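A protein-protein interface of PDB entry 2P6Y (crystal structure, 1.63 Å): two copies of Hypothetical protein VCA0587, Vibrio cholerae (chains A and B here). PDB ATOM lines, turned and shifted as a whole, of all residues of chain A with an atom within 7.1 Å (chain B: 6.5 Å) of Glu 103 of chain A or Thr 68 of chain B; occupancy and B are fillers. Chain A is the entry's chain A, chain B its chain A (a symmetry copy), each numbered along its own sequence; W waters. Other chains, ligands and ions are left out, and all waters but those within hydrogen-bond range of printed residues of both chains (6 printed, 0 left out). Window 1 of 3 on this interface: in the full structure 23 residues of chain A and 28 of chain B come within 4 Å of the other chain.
Of the 17 printed residues of chain A, 7 touch a printed residue of chain B. Of the 17 printed residues of chain B, 10 touch a printed residue of chain A. Among the printed residues, 17 pairs touch across the chains.
No position is printed for both chains. Of the 17 pairs that touch across the chains among the printed residues, none has its exchanged pair printed and touching as well.
Printed residues of chain B within 4 Å of Ala 6 of chain A: Phe 114. Of the printed residues of chain B, Met 105 of chain A touches Gly 31 (3.5 Å), Ser 32 (3.8 Å), Gly 67 (3.9 Å), Thr 68 (3.6 Å) and Phe 114 (3.9 Å). Of the printed residues of chain A, Gly 31 of chain B touches Met 105 (3.5 Å). Printed residues of chain A within 4 Å of Ser 66 of chain B: Val 37 (3.7 Å). The nearest printed residue of chain B that does not touch Ser 35 of chain A is Ser 66 of chain B (4.1 Å).
OG1 of Thr 68 of chain B is in hydrogen-bond range of OE1 of Glu 103 of chain A (2.6 Å). The side-chain carboxylate of Glu 103 of chain A is in hydrogen-bond range of a ring nitrogen (ND1) of His 75 of chain B (3.0 Å). OE2 of Glu 103 of chain A lies within salt-bridge range of NH1 of Arg 116 of chain B (3.1 Å).
Water W3 lies within hydrogen-bond range of the side-chain hydroxyl of Ser 35 of chain A, the backbone carbonyl oxygen of Glu 103 of chain A, the side-chain hydroxyl of Thr 68 of chain B and the backbone NH of Val 37 of chain A. Water W5 lies within hydrogen-bond range of the side-chain carboxylate of Glu 103 of chain A (2.7 Å), the side-chain carboxylate of Glu 126 of chain B (2.7 Å), the side-chain hydroxyl of Thr 101 of chain A (2.8 Å) and the backbone NH of Leu 127 of chain B (2.9 Å). Water W2 lies within hydrogen-bond range of O of Leu 127 of chain B (2.7 Å) and NH1 of Arg 8 of chain A (2.9 Å). Water W6 lies within hydrogen-bond range of the backbone carbonyl oxygen (O) of Ala 34 of chain A (2.8 Å), the backbone carbonyl oxygen (O) of Ile 33 of chain B (3.2 Å) and the side-chain hydroxyl (OG) of Ser 66 of chain B (3.4 Å). Water W1 lies within hydrogen-bond range of the backbone NH (N) of Gly 67 of chain B, the side-chain hydroxyl (OG) of Ser 35 of chain A and the backbone NH (N) of Ile 33 of chain B. Water W4 lies within hydrogen-bond range of the side-chain hydroxyl (OG) of Ser 32 of chain B (2.9 Å), the backbone carbonyl oxygen (O) of Ile 33 of chain B (3.3 Å) and the backbone carbonyl oxygen (O) of Ala 34 of chain A (3.5 Å).
Ala 6 of chain A touches Phe 114 of chain B. Glu 126 of chain B touches Arg 8 of chain A (CB to NH1, 3.3 Å). Leu 127 of chain B touches Arg 8 of chain A. O of Gly 67 of chain B touches OG of Ser 35 of chain A (3.6 Å). Val 37 of chain A touches Gly 67 of chain B (CG2 to CA, 3.6 Å). Met 105 of chain A touches Gly 31 of chain B (CE to O, 3.5 Å). Ser 32 of chain B touches Met 105 of chain A (CB to SD, 3.8 Å). CE of Met 105 of chain A touches O of Gly 67 of chain B, 3.9 Å away. Met 105 of chain A touches Thr 68 of chain B. Met 105 of chain A touches Phe 114 of chain B (CE to CE2, 3.9 Å).
The side-chain hydroxyl (OG1) of Thr 101 of chain A is in hydrogen-bond range of the guanidinium group (NE) of Arg 8 of chain A, 2.9 Å away. The backbone NH of Ala 34 of chain A lies within hydrogen-bond range of the backbone carbonyl oxygen of Met 105 of chain A (2.7 Å). N of Glu 103 of chain A lies within hydrogen-bond range of O of Val 37 of chain A (2.7 Å). The backbone NH (N) of Cys 39 of chain A lies within hydrogen-bond range of the backbone carbonyl oxygen (O) of Thr 101 of chain A (2.9 Å). NH2 of Arg 116 of chain B is in hydrogen-bond range of O of Ser 125 of chain B. The side-chain carboxylate (OE1) of Glu 126 of chain B lies within salt-bridge range of the guanidinium group (NH2) of Arg 116 of chain B, 3.7 Å away.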
ATOM      1  N   ALA A   6       6.081  -8.401  -2.953  1.00  0.00           N
ATOM      2  CA  ALA A   6       6.143  -7.210  -2.113  1.00  0.00           C
ATOM      3  C   ALA A   6       4.760  -6.818  -1.623  1.00  0.00           C
ATOM      4  O   ALA A   6       3.772  -6.951  -2.347  1.00  0.00           O
ATOM      5  CB  ALA A   6       6.765  -6.062  -2.889  1.00  0.00           C
ATOM      6  N   LEU A   7       4.697  -6.317  -0.393  1.00  0.00           N
ATOM      7  CA  LEU A   7       3.429  -5.927   0.204  1.00  0.00           C
ATOM      8  C   LEU A   7       3.648  -4.925   1.326  1.00  0.00           C
ATOM      9  O   LEU A   7       4.536  -5.112   2.157  1.00  0.00           O
ATOM     10  CB  LEU A   7       2.735  -7.171   0.770  1.00  0.00           C
ATOM     11  CG  LEU A   7       1.438  -7.037   1.579  1.00  0.00           C
ATOM     12  CD1 LEU A   7       0.298  -6.605   0.670  1.00  0.00           C
ATOM     13  CD2 LEU A   7       1.118  -8.374   2.234  1.00  0.00           C
ATOM     14  N   ARG A   8       2.861  -3.851   1.343  1.00  0.00           N
ATOM     15  CA  ARG A   8       2.979  -2.886   2.422  1.00  0.00           C
ATOM     16  C   ARG A   8       1.967  -3.295   3.482  1.00  0.00           C
ATOM     17  O   ARG A   8       0.801  -3.553   3.168  1.00  0.00           O
ATOM     18  CB  ARG A   8       2.655  -1.458   1.972  1.00  0.00           C
ATOM     19  CG  ARG A   8       2.786  -0.461   3.126  1.00  0.00           C
ATOM     20  CD  ARG A   8       1.917   0.775   2.985  1.00  0.00           C
ATOM     21  NE  ARG A   8       1.835   1.489   4.262  1.00  0.00           N
ATOM     22  CZ  ARG A   8       1.006   2.499   4.509  1.00  0.00           C
ATOM     23  NH1 ARG A   8       0.179   2.931   3.565  1.00  0.00           N
ATOM     24  NH2 ARG A   8       0.988   3.062   5.711  1.00  0.00           N
ATOM     25  N   LEU A   9       2.415  -3.376   4.731  1.00  0.00           N
ATOM     26  CA  LEU A   9       1.526  -3.724   5.832  1.00  0.00           C
ATOM     27  C   LEU A   9       1.148  -2.414   6.501  1.00  0.00           C
ATOM     28  O   LEU A   9       1.925  -1.454   6.476  1.00  0.00           O
ATOM     29  CB  LEU A   9       2.229  -4.648   6.832  1.00  0.00           C
ATOM     30  CG  LEU A   9       2.791  -5.943   6.244  1.00  0.00           C
ATOM     31  CD1 LEU A   9       3.352  -6.806   7.371  1.00  0.00           C
ATOM     32  CD2 LEU A   9       1.697  -6.690   5.489  1.00  0.00           C
ATOM     33  N   ALA A  34      13.397 -10.818   2.050  1.00  0.00           N
ATOM     34  CA  ALA A  34      14.328  -9.969   1.327  1.00  0.00           C
ATOM     35  C   ALA A  34      14.529  -8.635   2.037  1.00  0.00           C
ATOM     36  O   ALA A  34      15.644  -8.107   2.086  1.00  0.00           O
ATOM     37  CB  ALA A  34      13.816  -9.729  -0.088  1.00  0.00           C
ATOM     38  N   SER A  35      13.450  -8.090   2.588  1.00  0.00           N
ATOM     39  CA  SER A  35      13.525  -6.798   3.267  1.00  0.00           C
ATOM     40  C   SER A  35      12.249  -6.536   4.060  1.00  0.00           C
ATOM     41  O   SER A  35      11.191  -7.064   3.724  1.00  0.00           O
ATOM     42  CB  SER A  35      13.712  -5.692   2.217  1.00  0.00           C
ATOM     43  OG  SER A  35      13.911  -4.417   2.805  1.00  0.00           O
ATOM     44  N   CYS A  36      12.347  -5.740   5.124  1.00  0.00           N
ATOM     45  CA  CYS A  36      11.158  -5.399   5.900  1.00  0.00           C
ATOM     46  C   CYS A  36      11.281  -4.089   6.676  1.00  0.00           C
ATOM     47  O   CYS A  36      11.066  -4.048   7.890  1.00  0.00           O
ATOM     48  CB  CYS A  36      10.784  -6.524   6.866  1.00  0.00           C
ATOM     49  SG  CYS A  36       9.129  -6.293   7.574  1.00  0.00           S
ATOM     50  N   VAL A  37      11.615  -3.016   5.972  1.00  0.00           N
ATOM     51  CA  VAL A  37      11.753  -1.701   6.593  1.00  0.00           C
ATOM     52  C   VAL A  37      10.382  -1.282   7.132  1.00  0.00           C
ATOM     53  O   VAL A  37       9.372  -1.399   6.438  1.00  0.00           O
ATOM     54  CB  VAL A  37      12.234  -0.655   5.556  1.00  0.00           C
ATOM     55  CG1 VAL A  37      12.413   0.702   6.220  1.00  0.00           C
ATOM     56  CG2 VAL A  37      13.542  -1.117   4.916  1.00  0.00           C
ATOM     57  N   GLY A  38      10.342  -0.799   8.370  1.00  0.00           N
ATOM     58  CA  GLY A  38       9.074  -0.383   8.942  1.00  0.00           C
ATOM     59  C   GLY A  38       9.177  -0.144  10.430  1.00  0.00           C
ATOM     60  O   GLY A  38      10.275   0.011  10.958  1.00  0.00           O
ATOM     61  N   CYS A  39       8.035  -0.112  11.109  1.00  0.00           N
ATOM     62  CA  CYS A  39       8.031   0.114  12.548  1.00  0.00           C
ATOM     63  C   CYS A  39       6.894  -0.614  13.245  1.00  0.00           C
ATOM     64  O   CYS A  39       5.864  -0.925  12.639  1.00  0.00           O
ATOM     65  CB  CYS A  39       7.957   1.609  12.846  1.00  0.00           C
ATOM     66  SG  CYS A  39       6.686   2.482  11.929  1.00  0.00           S
ATOM     67  N   ILE A  62      11.977  -1.348  12.671  1.00  0.00           N
ATOM     68  CA  ILE A  62      12.404  -2.676  12.244  1.00  0.00           C
ATOM     69  C   ILE A  62      13.685  -2.478  11.432  1.00  0.00           C
ATOM     70  O   ILE A  62      13.670  -1.810  10.400  1.00  0.00           O
ATOM     71  CB  ILE A  62      11.345  -3.361  11.349  1.00  0.00           C
ATOM     72  CG1 ILE A  62      10.026  -3.490  12.112  1.00  0.00           C
ATOM     73  CG2 ILE A  62      11.853  -4.731  10.906  1.00  0.00           C
ATOM     74  CD1 ILE A  62       8.876  -4.059  11.284  1.00  0.00           C
ATOM     75  N   ILE A  98       2.217  -3.714  13.632  1.00  0.00           N
ATOM     76  CA  ILE A  98       2.723  -2.627  12.808  1.00  0.00           C
ATOM     77  C   ILE A  98       2.218  -1.285  13.325  1.00  0.00           C
ATOM     78  O   ILE A  98       1.058  -1.167  13.724  1.00  0.00           O
ATOM     79  CB  ILE A  98       2.251  -2.793  11.346  1.00  0.00           C
ATOM     80  CG1 ILE A  98       2.685  -4.162  10.816  1.00  0.00           C
ATOM     81  CG2 ILE A  98       2.784  -1.655  10.488  1.00  0.00           C
ATOM     82  CD1 ILE A  98       4.173  -4.446  10.959  1.00  0.00           C
ATOM     83  N   THR A 101       3.809   1.536   9.211  1.00  0.00           N
ATOM     84  CA  THR A 101       4.039   0.759   7.998  1.00  0.00           C
ATOM     85  C   THR A 101       5.110  -0.323   8.141  1.00  0.00           C
ATOM     86  O   THR A 101       5.918  -0.307   9.070  1.00  0.00           O
ATOM     87  CB  THR A 101       4.469   1.692   6.829  1.00  0.00           C
ATOM     88  OG1 THR A 101       4.356   0.996   5.582  1.00  0.00           O
ATOM     89  CG2 THR A 101       5.922   2.136   7.011  1.00  0.00           C
ATOM     90  N   ALA A 102       5.078  -1.268   7.209  1.00  0.00           N
ATOM     91  CA  ALA A 102       6.058  -2.345   7.109  1.00  0.00           C
ATOM     92  C   ALA A 102       6.126  -2.611   5.611  1.00  0.00           C
ATOM     93  O   ALA A 102       5.132  -3.001   4.994  1.00  0.00           O
ATOM     94  CB  ALA A 102       5.591  -3.600   7.854  1.00  0.00           C
ATOM     95  N   GLU A 103       7.289  -2.360   5.027  1.00  0.00           N
ATOM     96  CA  GLU A 103       7.498  -2.549   3.597  1.00  0.00           C
ATOM     97  C   GLU A 103       8.145  -3.914   3.406  1.00  0.00           C
ATOM     98  O   GLU A 103       9.362  -4.047   3.293  1.00  0.00           O
ATOM     99  CB  GLU A 103       8.370  -1.401   3.076  1.00  0.00           C
ATOM    100  CG  GLU A 103       7.637  -0.056   3.188  1.00  0.00           C
ATOM    101  CD  GLU A 103       8.542   1.166   3.115  1.00  0.00           C
ATOM    102  OE1 GLU A 103       9.706   1.041   2.687  1.00  0.00           O
ATOM    103  OE2 GLU A 103       8.076   2.266   3.478  1.00  0.00           O
ATOM    104  N   LEU A 104       7.291  -4.927   3.370  1.00  0.00           N
ATOM    105  CA  LEU A 104       7.706  -6.315   3.272  1.00  0.00           C
ATOM    106  C   LEU A 104       8.016  -6.843   1.878  1.00  0.00           C
ATOM    107  O   LEU A 104       7.242  -6.662   0.941  1.00  0.00           O
ATOM    108  CB  LEU A 104       6.627  -7.186   3.924  1.00  0.00           C
ATOM    109  CG  LEU A 104       6.804  -8.705   3.975  1.00  0.00           C
ATOM    110  CD1 LEU A 104       7.998  -9.064   4.852  1.00  0.00           C
ATOM    111  CD2 LEU A 104       5.529  -9.331   4.520  1.00  0.00           C
ATOM    112  N   MET A 105       9.166  -7.498   1.764  1.00  0.00           N
ATOM    113  CA  MET A 105       9.595  -8.111   0.518  1.00  0.00           C
ATOM    114  C   MET A 105      10.044  -9.532   0.799  1.00  0.00           C
ATOM    115  O   MET A 105      10.895  -9.772   1.652  1.00  0.00           O
ATOM    116  CB  MET A 105      10.735  -7.324  -0.101  1.00  0.00           C
ATOM    117  CG  MET A 105      10.306  -5.962  -0.549  1.00  0.00           C
ATOM    118  SD  MET A 105      11.666  -5.172  -1.608  1.00  0.00           S
ATOM    119  CE  MET A 105      11.738  -3.422  -0.805  1.00  0.00           C
ATOM    120  N   GLY B  31      13.520  -1.873  -5.875  1.00  0.00           N
ATOM    121  CA  GLY B  31      14.725  -2.572  -5.470  1.00  0.00           C
ATOM    122  C   GLY B  31      14.851  -2.684  -3.965  1.00  0.00           C
ATOM    123  O   GLY B  31      14.014  -2.172  -3.223  1.00  0.00           O
ATOM    124  N   SER B  32      15.901  -3.366  -3.525  1.00  0.00           N
ATOM    125  CA  SER B  32      16.171  -3.552  -2.106  1.00  0.00           C
ATOM    126  C   SER B  32      17.677  -3.691  -1.911  1.00  0.00           C
ATOM    127  O   SER B  32      18.429  -3.836  -2.879  1.00  0.00           O
ATOM    128  CB  SER B  32      15.462  -4.811  -1.587  1.00  0.00           C
ATOM    129  OG  SER B  32      15.969  -5.980  -2.215  1.00  0.00           O
ATOM    130  N   ILE B  33      18.121  -3.628  -0.660  1.00  0.00           N
ATOM    131  CA  ILE B  33      19.539  -3.772  -0.361  1.00  0.00           C
ATOM    132  C   ILE B  33      19.822  -5.243  -0.118  1.00  0.00           C
ATOM    133  O   ILE B  33      19.225  -5.859   0.765  1.00  0.00           O
ATOM    134  CB  ILE B  33      19.947  -2.999   0.914  1.00  0.00           C
ATOM    135  CG1 ILE B  33      19.586  -1.521   0.774  1.00  0.00           C
ATOM    136  CG2 ILE B  33      21.450  -3.163   1.155  1.00  0.00           C
ATOM    137  CD1 ILE B  33      20.325  -0.805  -0.343  1.00  0.00           C
ATOM    138  N   SER B  66      18.886  -2.447   5.401  1.00  0.00           N
ATOM    139  CA  SER B  66      17.673  -2.854   4.713  1.00  0.00           C
ATOM    140  C   SER B  66      17.095  -1.616   4.065  1.00  0.00           C
ATOM    141  O   SER B  66      17.175  -0.520   4.611  1.00  0.00           O
ATOM    142  CB  SER B  66      16.656  -3.446   5.693  1.00  0.00           C
ATOM    143  OG  SER B  66      17.142  -4.636   6.285  1.00  0.00           O
ATOM    144  N   GLY B  67      16.520  -1.775   2.884  1.00  0.00           N
ATOM    145  CA  GLY B  67      15.958  -0.608   2.248  1.00  0.00           C
ATOM    146  C   GLY B  67      14.968  -0.912   1.157  1.00  0.00           C
ATOM    147  O   GLY B  67      15.051  -1.940   0.493  1.00  0.00           O
ATOM    148  N   THR B  68      14.004  -0.012   1.014  1.00  0.00           N
ATOM    149  CA  THR B  68      13.004  -0.103  -0.035  1.00  0.00           C
ATOM    150  C   THR B  68      13.475   0.967  -1.004  1.00  0.00           C
ATOM    151  O   THR B  68      13.492   2.153  -0.669  1.00  0.00           O
ATOM    152  CB  THR B  68      11.606   0.265   0.477  1.00  0.00           C
ATOM    153  OG1 THR B  68      11.189  -0.693   1.457  1.00  0.00           O
ATOM    154  CG2 THR B  68      10.606   0.279  -0.676  1.00  0.00           C
ATOM    155  N   LEU B  69      13.884   0.550  -2.194  1.00  0.00           N
ATOM    156  CA  LEU B  69      14.376   1.503  -3.175  1.00  0.00           C
ATOM    157  C   LEU B  69      13.347   1.821  -4.252  1.00  0.00           C
ATOM    158  O   LEU B  69      12.778   0.917  -4.870  1.00  0.00           O
ATOM    159  CB  LEU B  69      15.653   0.969  -3.835  1.00  0.00           C
ATOM    160  CG  LEU B  69      16.713   0.380  -2.895  1.00  0.00           C
ATOM    161  CD1 LEU B  69      17.897  -0.127  -3.700  1.00  0.00           C
ATOM    162  CD2 LEU B  69      17.162   1.430  -1.894  1.00  0.00           C
ATOM    163  N   THR B  70      13.096   3.115  -4.436  1.00  0.00           N
ATOM    164  CA  THR B  70      12.186   3.613  -5.469  1.00  0.00           C
ATOM    165  C   THR B  70      13.001   4.727  -6.100  1.00  0.00           C
ATOM    166  O   THR B  70      13.934   5.245  -5.480  1.00  0.00           O
ATOM    167  CB  THR B  70      10.871   4.203  -4.905  1.00  0.00           C
ATOM    168  OG1 THR B  70      11.114   5.506  -4.360  1.00  0.00           O
ATOM    169  CG2 THR B  70      10.295   3.294  -3.827  1.00  0.00           C
ATOM    170  N   HIS B  73      12.677   7.920  -3.927  1.00  0.00           N
ATOM    171  CA  HIS B  73      12.903   7.826  -2.493  1.00  0.00           C
ATOM    172  C   HIS B  73      13.460   6.485  -2.044  1.00  0.00           C
ATOM    173  O   HIS B  73      12.992   5.434  -2.475  1.00  0.00           O
ATOM    174  CB  HIS B  73      11.581   8.075  -1.762  1.00  0.00           C
ATOM    175  CG  HIS B  73      11.682   7.979  -0.270  1.00  0.00           C
ATOM    176  ND1 HIS B  73      11.931   9.072   0.532  1.00  0.00           N
ATOM    177  CD2 HIS B  73      11.561   6.920   0.565  1.00  0.00           C
ATOM    178  CE1 HIS B  73      11.956   8.691   1.797  1.00  0.00           C
ATOM    179  NE2 HIS B  73      11.734   7.390   1.844  1.00  0.00           N
ATOM    180  N   CYS B  74      14.455   6.535  -1.164  1.00  0.00           N
ATOM    181  CA  CYS B  74      15.051   5.325  -0.612  1.00  0.00           C
ATOM    182  C   CYS B  74      14.806   5.340   0.891  1.00  0.00           C
ATOM    183  O   CYS B  74      15.238   6.263   1.586  1.00  0.00           O
ATOM    184  CB  CYS B  74      16.551   5.274  -0.899  1.00  0.00           C
ATOM    185  SG  CYS B  74      16.959   4.943  -2.629  1.00  0.00           S
ATOM    186  N   HIS B  75      14.094   4.325   1.376  1.00  0.00           N
ATOM    187  CA  HIS B  75      13.764   4.192   2.793  1.00  0.00           C
ATOM    188  C   HIS B  75      14.726   3.152   3.353  1.00  0.00           C
ATOM    189  O   HIS B  75      14.529   1.951   3.173  1.00  0.00           O
ATOM    190  CB  HIS B  75      12.318   3.717   2.950  1.00  0.00           C
ATOM    191  CG  HIS B  75      11.801   3.816   4.351  1.00  0.00           C
ATOM    192  ND1 HIS B  75      10.541   3.390   4.713  1.00  0.00           N
ATOM    193  CD2 HIS B  75      12.370   4.307   5.475  1.00  0.00           C
ATOM    194  CE1 HIS B  75      10.355   3.619   6.001  1.00  0.00           C
ATOM    195  NE2 HIS B  75      11.450   4.175   6.487  1.00  0.00           N
ATOM    196  N   LEU B  76      15.760   3.629   4.038  1.00  0.00           N
ATOM    197  CA  LEU B  76      16.806   2.761   4.567  1.00  0.00           C
ATOM    198  C   LEU B  76      16.945   2.718   6.086  1.00  0.00           C
ATOM    199  O   LEU B  76      16.944   3.755   6.745  1.00  0.00           O
ATOM    200  CB  LEU B  76      18.149   3.194   3.977  1.00  0.00           C
ATOM    201  CG  LEU B  76      18.315   3.150   2.454  1.00  0.00           C
ATOM    202  CD1 LEU B  76      19.338   4.189   1.995  1.00  0.00           C
ATOM    203  CD2 LEU B  76      18.742   1.756   2.049  1.00  0.00           C
ATOM    204  N   PHE B 114       7.799   0.402  -7.706  1.00  0.00           N
ATOM    205  CA  PHE B 114       7.459   0.879  -6.371  1.00  0.00           C
ATOM    206  C   PHE B 114       7.343   2.392  -6.418  1.00  0.00           C
ATOM    207  O   PHE B 114       8.190   3.065  -7.003  1.00  0.00           O
ATOM    208  CB  PHE B 114       8.549   0.556  -5.345  1.00  0.00           C
ATOM    209  CG  PHE B 114       8.806  -0.911  -5.139  1.00  0.00           C
ATOM    210  CD1 PHE B 114       7.840  -1.868  -5.438  1.00  0.00           C
ATOM    211  CD2 PHE B 114      10.017  -1.331  -4.598  1.00  0.00           C
ATOM    212  CE1 PHE B 114       8.086  -3.229  -5.199  1.00  0.00           C
ATOM    213  CE2 PHE B 114      10.272  -2.682  -4.356  1.00  0.00           C
ATOM    214  CZ  PHE B 114       9.304  -3.631  -4.657  1.00  0.00           C
ATOM    215  N   ARG B 116       5.537   5.955  -3.980  1.00  0.00           N
ATOM    216  CA  ARG B 116       5.111   6.348  -2.647  1.00  0.00           C
ATOM    217  C   ARG B 116       4.020   7.406  -2.773  1.00  0.00           C
ATOM    218  O   ARG B 116       4.161   8.373  -3.524  1.00  0.00           O
ATOM    219  CB  ARG B 116       6.299   6.875  -1.836  1.00  0.00           C
ATOM    220  CG  ARG B 116       7.400   5.835  -1.618  1.00  0.00           C
ATOM    221  CD  ARG B 116       8.465   6.328  -0.647  1.00  0.00           C
ATOM    222  NE  ARG B 116       8.011   6.304   0.745  1.00  0.00           N
ATOM    223  CZ  ARG B 116       8.146   5.262   1.563  1.00  0.00           C
ATOM    224  NH1 ARG B 116       8.727   4.148   1.135  1.00  0.00           N
ATOM    225  NH2 ARG B 116       7.699   5.332   2.809  1.00  0.00           N
ATOM    226  N   SER B 125       4.474   9.780   3.234  1.00  0.00           N
ATOM    227  CA  SER B 125       4.253   9.169   1.929  1.00  0.00           C
ATOM    228  C   SER B 125       4.599   7.705   2.181  1.00  0.00           C
ATOM    229  O   SER B 125       5.644   7.412   2.763  1.00  0.00           O
ATOM    230  CB  SER B 125       5.204   9.757   0.886  1.00  0.00           C
ATOM    231  OG  SER B 125       5.042  11.161   0.781  1.00  0.00           O
ATOM    232  N   GLU B 126       3.731   6.790   1.764  1.00  0.00           N
ATOM    233  CA  GLU B 126       3.977   5.372   2.002  1.00  0.00           C
ATOM    234  C   GLU B 126       4.089   4.542   0.727  1.00  0.00           C
ATOM    235  O   GLU B 126       3.592   4.928  -0.334  1.00  0.00           O
ATOM    236  CB  GLU B 126       2.872   4.802   2.894  1.00  0.00           C
ATOM    237  CG  GLU B 126       2.622   5.589   4.178  1.00  0.00           C
ATOM    238  CD  GLU B 126       3.739   5.464   5.209  1.00  0.00           C
ATOM    239  OE1 GLU B 126       4.735   4.751   4.955  1.00  0.00           O
ATOM    240  OE2 GLU B 126       3.609   6.087   6.285  1.00  0.00           O
ATOM    241  N   LEU B 127       4.733   3.386   0.849  1.00  0.00           N
ATOM    242  CA  LEU B 127       4.951   2.480  -0.272  1.00  0.00           C
ATOM    243  C   LEU B 127       3.692   1.970  -0.959  1.00  0.00           C
ATOM    244  O   LEU B 127       2.731   1.561  -0.309  1.00  0.00           O
ATOM    245  CB  LEU B 127       5.774   1.269   0.187  1.00  0.00           C
ATOM    246  CG  LEU B 127       5.989   0.154  -0.843  1.00  0.00           C
ATOM    247  CD1 LEU B 127       6.937   0.628  -1.936  1.00  0.00           C
ATOM    248  CD2 LEU B 127       6.562  -1.080  -0.147  1.00  0.00           C
HETATM  249  O   HOH W   1      16.653  -4.424   1.779  1.00  0.00           O
HETATM  250  O   HOH W   2       0.548   2.893   0.658  1.00  0.00           O
HETATM  251  O   HOH W   3      11.744  -3.017   2.764  1.00  0.00           O
HETATM  252  O   HOH W   4      17.414  -8.111  -0.928  1.00  0.00           O
HETATM  253  O   HOH W   5       5.440   2.558   3.544  1.00  0.00           O
HETATM  254  O   HOH W   6      17.459  -6.372   3.427  1.00  0.00           O
